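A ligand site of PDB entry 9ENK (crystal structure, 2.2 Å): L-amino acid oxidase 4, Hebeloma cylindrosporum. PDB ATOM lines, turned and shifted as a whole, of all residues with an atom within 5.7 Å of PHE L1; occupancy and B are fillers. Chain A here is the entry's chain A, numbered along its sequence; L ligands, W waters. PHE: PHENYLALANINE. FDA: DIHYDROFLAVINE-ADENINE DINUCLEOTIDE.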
ATOM      1  N   MET A  69     -27.153  23.561 -24.736  1.00  0.00           N
ATOM      2  CA  MET A  69     -28.270  23.804 -23.826  1.00  0.00           C
ATOM      3  C   MET A  69     -28.568  25.268 -23.528  1.00  0.00           C
ATOM      4  O   MET A  69     -29.670  25.547 -23.044  1.00  0.00           O
ATOM      5  CB  MET A  69     -28.016  23.078 -22.481  1.00  0.00           C
ATOM      6  CG  MET A  69     -26.901  23.681 -21.651  1.00  0.00           C
ATOM      7  SD  MET A  69     -26.618  22.781 -20.084  1.00  0.00           S
ATOM      8  CE  MET A  69     -25.436  23.867 -19.292  1.00  0.00           C
ATOM      9  N   ARG A  70     -27.667  26.211 -23.813  1.00  0.00           N
ATOM     10  CA  ARG A  70     -27.864  27.595 -23.426  1.00  0.00           C
ATOM     11  C   ARG A  70     -27.275  28.524 -24.480  1.00  0.00           C
ATOM     12  O   ARG A  70     -26.234  28.229 -25.059  1.00  0.00           O
ATOM     13  CB  ARG A  70     -27.233  27.885 -22.064  1.00  0.00           C
ATOM     14  CG  ARG A  70     -25.752  27.592 -21.991  1.00  0.00           C
ATOM     15  CD  ARG A  70     -25.255  27.618 -20.548  1.00  0.00           C
ATOM     16  NE  ARG A  70     -23.869  27.196 -20.444  1.00  0.00           N
ATOM     17  CZ  ARG A  70     -23.237  26.985 -19.297  1.00  0.00           C
ATOM     18  NH1 ARG A  70     -23.831  27.147 -18.133  1.00  0.00           N
ATOM     19  NH2 ARG A  70     -21.958  26.608 -19.329  1.00  0.00           N
ATOM     20  N   TRP A 224      -7.532  24.073 -18.099  1.00  0.00           N
ATOM     21  CA  TRP A 224      -7.969  25.074 -19.076  1.00  0.00           C
ATOM     22  C   TRP A 224      -6.831  26.019 -19.457  1.00  0.00           C
ATOM     23  O   TRP A 224      -6.653  26.366 -20.641  1.00  0.00           O
ATOM     24  CB  TRP A 224      -9.148  25.861 -18.505  1.00  0.00           C
ATOM     25  CG  TRP A 224      -9.680  26.940 -19.398  1.00  0.00           C
ATOM     26  CD1 TRP A 224      -9.056  28.101 -19.762  1.00  0.00           C
ATOM     27  CD2 TRP A 224     -10.975  26.966 -20.032  1.00  0.00           C
ATOM     28  NE1 TRP A 224      -9.878  28.848 -20.574  1.00  0.00           N
ATOM     29  CE2 TRP A 224     -11.052  28.170 -20.757  1.00  0.00           C
ATOM     30  CE3 TRP A 224     -12.072  26.100 -20.037  1.00  0.00           C
ATOM     31  CZ2 TRP A 224     -12.183  28.512 -21.493  1.00  0.00           C
ATOM     32  CZ3 TRP A 224     -13.189  26.444 -20.772  1.00  0.00           C
ATOM     33  CH2 TRP A 224     -13.231  27.645 -21.483  1.00  0.00           C
ATOM     34  N   GLU A 235     -13.592  32.619 -25.686  1.00  0.00           N
ATOM     35  CA  GLU A 235     -14.700  32.075 -24.924  1.00  0.00           C
ATOM     36  C   GLU A 235     -15.217  33.081 -23.910  1.00  0.00           C
ATOM     37  O   GLU A 235     -16.422  33.133 -23.638  1.00  0.00           O
ATOM     38  CB  GLU A 235     -14.292  30.774 -24.246  1.00  0.00           C
ATOM     39  CG  GLU A 235     -13.880  29.673 -25.232  1.00  0.00           C
ATOM     40  CD  GLU A 235     -15.014  29.212 -26.117  1.00  0.00           C
ATOM     41  OE1 GLU A 235     -16.157  29.699 -25.929  1.00  0.00           O
ATOM     42  OE2 GLU A 235     -14.769  28.359 -27.023  1.00  0.00           O
ATOM     43  N   PHE A 239     -19.092  33.858 -23.795  1.00  0.00           N
ATOM     44  CA  PHE A 239     -19.871  33.784 -22.568  1.00  0.00           C
ATOM     45  C   PHE A 239     -20.338  35.155 -22.097  1.00  0.00           C
ATOM     46  O   PHE A 239     -21.129  35.216 -21.146  1.00  0.00           O
ATOM     47  CB  PHE A 239     -19.065  33.155 -21.435  1.00  0.00           C
ATOM     48  CG  PHE A 239     -19.132  31.664 -21.396  1.00  0.00           C
ATOM     49  CD1 PHE A 239     -20.270  31.026 -20.952  1.00  0.00           C
ATOM     50  CD2 PHE A 239     -18.045  30.901 -21.776  1.00  0.00           C
ATOM     51  CE1 PHE A 239     -20.337  29.649 -20.913  1.00  0.00           C
ATOM     52  CE2 PHE A 239     -18.096  29.512 -21.734  1.00  0.00           C
ATOM     53  CZ  PHE A 239     -19.242  28.892 -21.313  1.00  0.00           C
ATOM     54  N   TRP A 249     -29.706  35.336 -21.991  1.00  0.00           N
ATOM     55  CA  TRP A 249     -29.551  33.886 -21.932  1.00  0.00           C
ATOM     56  C   TRP A 249     -30.878  33.213 -22.242  1.00  0.00           C
ATOM     57  O   TRP A 249     -31.894  33.488 -21.607  1.00  0.00           O
ATOM     58  CB  TRP A 249     -29.042  33.456 -20.556  1.00  0.00           C
ATOM     59  CG  TRP A 249     -27.573  33.684 -20.342  1.00  0.00           C
ATOM     60  CD1 TRP A 249     -27.005  34.695 -19.618  1.00  0.00           C
ATOM     61  CD2 TRP A 249     -26.494  32.913 -20.864  1.00  0.00           C
ATOM     62  NE1 TRP A 249     -25.643  34.584 -19.656  1.00  0.00           N
ATOM     63  CE2 TRP A 249     -25.305  33.492 -20.408  1.00  0.00           C
ATOM     64  CE3 TRP A 249     -26.415  31.771 -21.679  1.00  0.00           C
ATOM     65  CZ2 TRP A 249     -24.039  32.984 -20.732  1.00  0.00           C
ATOM     66  CZ3 TRP A 249     -25.179  31.260 -21.996  1.00  0.00           C
ATOM     67  CH2 TRP A 249     -24.001  31.862 -21.524  1.00  0.00           C
ATOM     68  N   TYR A 404     -21.153  18.527 -14.945  1.00  0.00           N
ATOM     69  CA  TYR A 404     -20.788  19.031 -16.276  1.00  0.00           C
ATOM     70  C   TYR A 404     -19.333  19.473 -16.184  1.00  0.00           C
ATOM     71  O   TYR A 404     -19.036  20.468 -15.527  1.00  0.00           O
ATOM     72  CB  TYR A 404     -21.716  20.172 -16.691  1.00  0.00           C
ATOM     73  CG  TYR A 404     -21.385  20.791 -18.036  1.00  0.00           C
ATOM     74  CD1 TYR A 404     -20.653  20.100 -18.996  1.00  0.00           C
ATOM     75  CD2 TYR A 404     -21.806  22.080 -18.331  1.00  0.00           C
ATOM     76  CE1 TYR A 404     -20.342  20.673 -20.218  1.00  0.00           C
ATOM     77  CE2 TYR A 404     -21.511  22.665 -19.555  1.00  0.00           C
ATOM     78  CZ  TYR A 404     -20.779  21.962 -20.494  1.00  0.00           C
ATOM     79  OH  TYR A 404     -20.472  22.551 -21.697  1.00  0.00           O
ATOM     80  N   TRP A 406     -15.137  19.794 -17.851  1.00  0.00           N
ATOM     81  CA  TRP A 406     -14.270  20.118 -18.960  1.00  0.00           C
ATOM     82  C   TRP A 406     -12.847  19.604 -18.682  1.00  0.00           C
ATOM     83  O   TRP A 406     -12.521  19.176 -17.568  1.00  0.00           O
ATOM     84  CB  TRP A 406     -14.216  21.630 -19.195  1.00  0.00           C
ATOM     85  CG  TRP A 406     -15.511  22.246 -19.600  1.00  0.00           C
ATOM     86  CD1 TRP A 406     -16.519  21.648 -20.288  1.00  0.00           C
ATOM     87  CD2 TRP A 406     -15.933  23.590 -19.355  1.00  0.00           C
ATOM     88  NE1 TRP A 406     -17.544  22.536 -20.488  1.00  0.00           N
ATOM     89  CE2 TRP A 406     -17.206  23.740 -19.927  1.00  0.00           C
ATOM     90  CE3 TRP A 406     -15.346  24.688 -18.708  1.00  0.00           C
ATOM     91  CZ2 TRP A 406     -17.921  24.946 -19.881  1.00  0.00           C
ATOM     92  CZ3 TRP A 406     -16.047  25.896 -18.661  1.00  0.00           C
ATOM     93  CH2 TRP A 406     -17.323  26.009 -19.240  1.00  0.00           C
ATOM     94  N   PHE A 469     -15.462  19.208 -28.514  1.00  0.00           N
ATOM     95  CA  PHE A 469     -15.439  20.330 -29.443  1.00  0.00           C
ATOM     96  C   PHE A 469     -13.992  20.789 -29.595  1.00  0.00           C
ATOM     97  O   PHE A 469     -13.109  20.402 -28.830  1.00  0.00           O
ATOM     98  CB  PHE A 469     -16.325  21.484 -28.956  1.00  0.00           C
ATOM     99  CG  PHE A 469     -16.394  21.603 -27.460  1.00  0.00           C
ATOM    100  CD1 PHE A 469     -15.273  21.932 -26.726  1.00  0.00           C
ATOM    101  CD2 PHE A 469     -17.592  21.397 -26.790  1.00  0.00           C
ATOM    102  CE1 PHE A 469     -15.330  22.040 -25.348  1.00  0.00           C
ATOM    103  CE2 PHE A 469     -17.663  21.516 -25.425  1.00  0.00           C
ATOM    104  CZ  PHE A 469     -16.532  21.825 -24.698  1.00  0.00           C
ATOM    105  N   PHE A 471     -10.875  22.879 -29.055  1.00  0.00           N
ATOM    106  CA  PHE A 471     -10.330  23.643 -27.927  1.00  0.00           C
ATOM    107  C   PHE A 471      -8.835  23.795 -28.198  1.00  0.00           C
ATOM    108  O   PHE A 471      -8.003  23.037 -27.707  1.00  0.00           O
ATOM    109  CB  PHE A 471     -10.612  22.972 -26.582  1.00  0.00           C
ATOM    110  CG  PHE A 471     -10.398  23.884 -25.392  1.00  0.00           C
ATOM    111  CD1 PHE A 471      -9.745  25.102 -25.526  1.00  0.00           C
ATOM    112  CD2 PHE A 471     -10.835  23.501 -24.140  1.00  0.00           C
ATOM    113  CE1 PHE A 471      -9.555  25.930 -24.431  1.00  0.00           C
ATOM    114  CE2 PHE A 471     -10.651  24.322 -23.046  1.00  0.00           C
ATOM    115  CZ  PHE A 471     -10.012  25.537 -23.181  1.00  0.00           C
ATOM    116  N   HIS A 504     -15.555  28.310 -30.989  1.00  0.00           N
ATOM    117  CA  HIS A 504     -15.540  26.884 -30.684  1.00  0.00           C
ATOM    118  C   HIS A 504     -16.472  26.587 -29.523  1.00  0.00           C
ATOM    119  O   HIS A 504     -16.627  27.382 -28.593  1.00  0.00           O
ATOM    120  CB  HIS A 504     -14.114  26.432 -30.361  1.00  0.00           C
ATOM    121  CG  HIS A 504     -13.182  26.500 -31.531  1.00  0.00           C
ATOM    122  ND1 HIS A 504     -11.833  26.721 -31.399  1.00  0.00           N
ATOM    123  CD2 HIS A 504     -13.420  26.372 -32.857  1.00  0.00           C
ATOM    124  CE1 HIS A 504     -11.269  26.709 -32.590  1.00  0.00           C
ATOM    125  NE2 HIS A 504     -12.210  26.504 -33.499  1.00  0.00           N
ATOM    126  N   ALA A 505     -17.112  25.422 -29.594  1.00  0.00           N
ATOM    127  CA  ALA A 505     -18.011  24.944 -28.554  1.00  0.00           C
ATOM    128  C   ALA A 505     -19.303  25.765 -28.494  1.00  0.00           C
ATOM    129  O   ALA A 505     -19.947  25.838 -27.448  1.00  0.00           O
ATOM    130  CB  ALA A 505     -17.321  24.919 -27.187  1.00  0.00           C
ATOM    131  N   TRP A 506     -19.675  26.396 -29.601  1.00  0.00           N
ATOM    132  CA  TRP A 506     -20.921  27.128 -29.689  1.00  0.00           C
ATOM    133  C   TRP A 506     -21.622  26.792 -31.004  1.00  0.00           C
ATOM    134  O   TRP A 506     -20.973  26.461 -31.996  1.00  0.00           O
ATOM    135  CB  TRP A 506     -20.698  28.649 -29.603  1.00  0.00           C
ATOM    136  CG  TRP A 506     -20.182  29.093 -28.287  1.00  0.00           C
ATOM    137  CD1 TRP A 506     -18.881  29.392 -27.976  1.00  0.00           C
ATOM    138  CD2 TRP A 506     -20.932  29.278 -27.091  1.00  0.00           C
ATOM    139  NE1 TRP A 506     -18.790  29.752 -26.667  1.00  0.00           N
ATOM    140  CE2 TRP A 506     -20.032  29.695 -26.096  1.00  0.00           C
ATOM    141  CE3 TRP A 506     -22.284  29.140 -26.767  1.00  0.00           C
ATOM    142  CZ2 TRP A 506     -20.440  29.979 -24.791  1.00  0.00           C
ATOM    143  CZ3 TRP A 506     -22.692  29.436 -25.474  1.00  0.00           C
ATOM    144  CH2 TRP A 506     -21.768  29.848 -24.495  1.00  0.00           C
HETATM  145  N   PHE L   1     -20.885  26.731 -24.943  1.00  0.00           N
HETATM  146  CA  PHE L   1     -20.955  25.594 -24.038  1.00  0.00           C
HETATM  147  C   PHE L   1     -21.312  26.017 -22.610  1.00  0.00           C
HETATM  148  O   PHE L   1     -21.807  27.114 -22.410  1.00  0.00           O
HETATM  149  CB  PHE L   1     -19.641  24.795 -24.048  1.00  0.00           C
HETATM  150  CG  PHE L   1     -18.373  25.591 -23.795  1.00  0.00           C
HETATM  151  CD1 PHE L   1     -18.206  26.884 -24.260  1.00  0.00           C
HETATM  152  CD2 PHE L   1     -17.326  24.996 -23.135  1.00  0.00           C
HETATM  153  CE1 PHE L   1     -17.037  27.567 -24.028  1.00  0.00           C
HETATM  154  CE2 PHE L   1     -16.157  25.679 -22.903  1.00  0.00           C
HETATM  155  CZ  PHE L   1     -16.013  26.964 -23.350  1.00  0.00           C
HETATM  156  OXT PHE L   1     -21.162  25.230 -21.673  1.00  0.00           O
HETATM  157  PA  FDA L   2     -21.899  18.029 -35.062  1.00  0.00           P
HETATM  158  O1A FDA L   2     -20.928  17.086 -34.439  1.00  0.00           O
HETATM  159  O2A FDA L   2     -23.038  18.519 -34.228  1.00  0.00           O
HETATM  160  O5B FDA L   2     -22.500  17.346 -36.386  1.00  0.00           O
HETATM  161  C5B FDA L   2     -21.680  16.459 -37.187  1.00  0.00           C
HETATM  162  C4B FDA L   2     -22.559  15.377 -37.786  1.00  0.00           C
HETATM  163  O4B FDA L   2     -21.737  14.451 -38.563  1.00  0.00           O
HETATM  164  C3B FDA L   2     -23.315  14.504 -36.775  1.00  0.00           C
HETATM  165  O3B FDA L   2     -24.671  14.301 -37.152  1.00  0.00           O
HETATM  166  C2B FDA L   2     -22.562  13.166 -36.825  1.00  0.00           C
HETATM  167  O2B FDA L   2     -23.373  12.077 -36.467  1.00  0.00           O
HETATM  168  C1B FDA L   2     -22.139  13.112 -38.280  1.00  0.00           C
HETATM  169  N9A FDA L   2     -21.041  12.264 -38.601  1.00  0.00           N
HETATM  170  C8A FDA L   2     -19.948  11.965 -37.822  1.00  0.00           C
HETATM  171  N7A FDA L   2     -19.114  11.158 -38.427  1.00  0.00           N
HETATM  172  C5A FDA L   2     -19.681  10.908 -39.675  1.00  0.00           C
HETATM  173  C6A FDA L   2     -19.278  10.132 -40.763  1.00  0.00           C
HETATM  174  N6A FDA L   2     -18.144   9.424 -40.800  1.00  0.00           N
HETATM  175  N1A FDA L   2     -20.081  10.109 -41.845  1.00  0.00           N
HETATM  176  C2A FDA L   2     -21.222  10.823 -41.809  1.00  0.00           C
HETATM  177  N3A FDA L   2     -21.706  11.586 -40.840  1.00  0.00           N
HETATM  178  C4A FDA L   2     -20.876  11.587 -39.783  1.00  0.00           C
HETATM  179  N1  FDA L   2     -23.296  25.285 -28.164  1.00  0.00           N
HETATM  180  C2  FDA L   2     -24.133  26.322 -27.823  1.00  0.00           C
HETATM  181  O2  FDA L   2     -24.452  27.168 -28.631  1.00  0.00           O
HETATM  182  N3  FDA L   2     -24.575  26.351 -26.519  1.00  0.00           N
HETATM  183  C4  FDA L   2     -24.235  25.439 -25.541  1.00  0.00           C
HETATM  184  O4  FDA L   2     -24.700  25.562 -24.410  1.00  0.00           O
HETATM  185  C4X FDA L   2     -23.367  24.403 -25.909  1.00  0.00           C
HETATM  186  N5  FDA L   2     -22.965  23.453 -25.012  1.00  0.00           N
HETATM  187  C5X FDA L   2     -22.290  22.315 -25.401  1.00  0.00           C
HETATM  188  C6  FDA L   2     -22.062  21.274 -24.514  1.00  0.00           C
HETATM  189  C7  FDA L   2     -21.410  20.140 -24.896  1.00  0.00           C
HETATM  190  C7M FDA L   2     -21.182  19.024 -23.911  1.00  0.00           C
HETATM  191  C8  FDA L   2     -20.972  20.011 -26.261  1.00  0.00           C
HETATM  192  C8M FDA L   2     -20.263  18.755 -26.717  1.00  0.00           C
HETATM  193  C9  FDA L   2     -21.206  21.032 -27.137  1.00  0.00           C
HETATM  194  C9A FDA L   2     -21.857  22.203 -26.738  1.00  0.00           C
HETATM  195  N10 FDA L   2     -22.076  23.287 -27.629  1.00  0.00           N
HETATM  196  C10 FDA L   2     -22.916  24.327 -27.258  1.00  0.00           C
HETATM  197  C1' FDA L   2     -21.438  23.306 -28.957  1.00  0.00           C
HETATM  198  C2' FDA L   2     -22.374  22.789 -30.048  1.00  0.00           C
HETATM  199  O2' FDA L   2     -23.064  21.655 -29.552  1.00  0.00           O
HETATM  200  C3' FDA L   2     -21.527  22.413 -31.267  1.00  0.00           C
HETATM  201  O3' FDA L   2     -20.513  23.419 -31.475  1.00  0.00           O
HETATM  202  C4' FDA L   2     -22.322  22.254 -32.568  1.00  0.00           C
HETATM  203  O4' FDA L   2     -23.524  21.563 -32.288  1.00  0.00           O
HETATM  204  C5' FDA L   2     -21.512  21.500 -33.595  1.00  0.00           C
HETATM  205  O5' FDA L   2     -22.266  21.347 -34.811  1.00  0.00           O
HETATM  206  P   FDA L   2     -21.530  20.766 -36.104  1.00  0.00           P
HETATM  207  O1P FDA L   2     -22.551  20.648 -37.180  1.00  0.00           O
HETATM  208  O2P FDA L   2     -20.297  21.572 -36.331  1.00  0.00           O
HETATM  209  O3P FDA L   2     -21.090  19.297 -35.629  1.00  0.00           O
HETATM  210  O   HOH W   1     -13.408  25.389 -24.152  1.00  0.00           O
HETATM  211  O   HOH W   2     -13.940  23.222 -22.413  1.00  0.00           O
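Trp 224 touches PHE L1.
OE1 of Glu 235 touches CE1 of PHE L1 (3.0 Å).
Phe 239 touches PHE L1.
CZ2 of Trp 406 touches CD2 of PHE L1 (3.3 Å).
Phe 469 touches PHE L1.
Trp 506 touches PHE L1.
Hydrophobic or aromatic side chains within 4 Å of PHE L1: Trp 224, Phe 239, Tyr 404, Trp 406, Phe 469, Ala 505 and Trp 506.
Of the 13 residues printed, 9 come within 4 Å of PHE L1.
Along chain A the residues within 4 Å of PHE L1 span positions 70 to 506.
The side-chain hydroxyl of Tyr 404 sits at hydrogen-bond distance from the indole nitrogen of Trp 406 (3.2 Å).
The indole nitrogen (NE1) of Trp 506 sits at hydrogen-bond distance from the side-chain carboxylate (OE1) of Glu 235 (2.7 Å).
The side-chain carboxylate (OE2) of Glu 235 lies close to the backbone carbonyl oxygen (O) of His 504 (2.6 Å).
O of Arg 70 sits at hydrogen-bond distance from N3 of FDA L2 (2.9 Å).
The backbone carbonyl oxygen (O) of Ala 505 lies close to a nitrogen (N1) of FDA L2.
An oxygen (OXT) of PHE L1 lies within hydrogen-bond range of the side-chain hydroxyl of Tyr 404 (2.8 Å).
The backbone carbonyl oxygen (O) of Trp 506 lies within hydrogen-bond range of an oxygen (O3') of FDA L2 (3.1 Å).
An oxygen (O4) of FDA L2 is in hydrogen-bond range of the backbone NH of Met 69, 3.2 Å away.
OXT of PHE L1 lies within salt-bridge range of NH2 of Arg 70, 2.8 Å away.
A nitrogen (N) of PHE L1 lies within hydrogen-bond range of the backbone carbonyl oxygen of Ala 505 (2.8 Å).
N of Arg 70 lies within hydrogen-bond range of O4 of FDA L2, at 3.1 Å.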
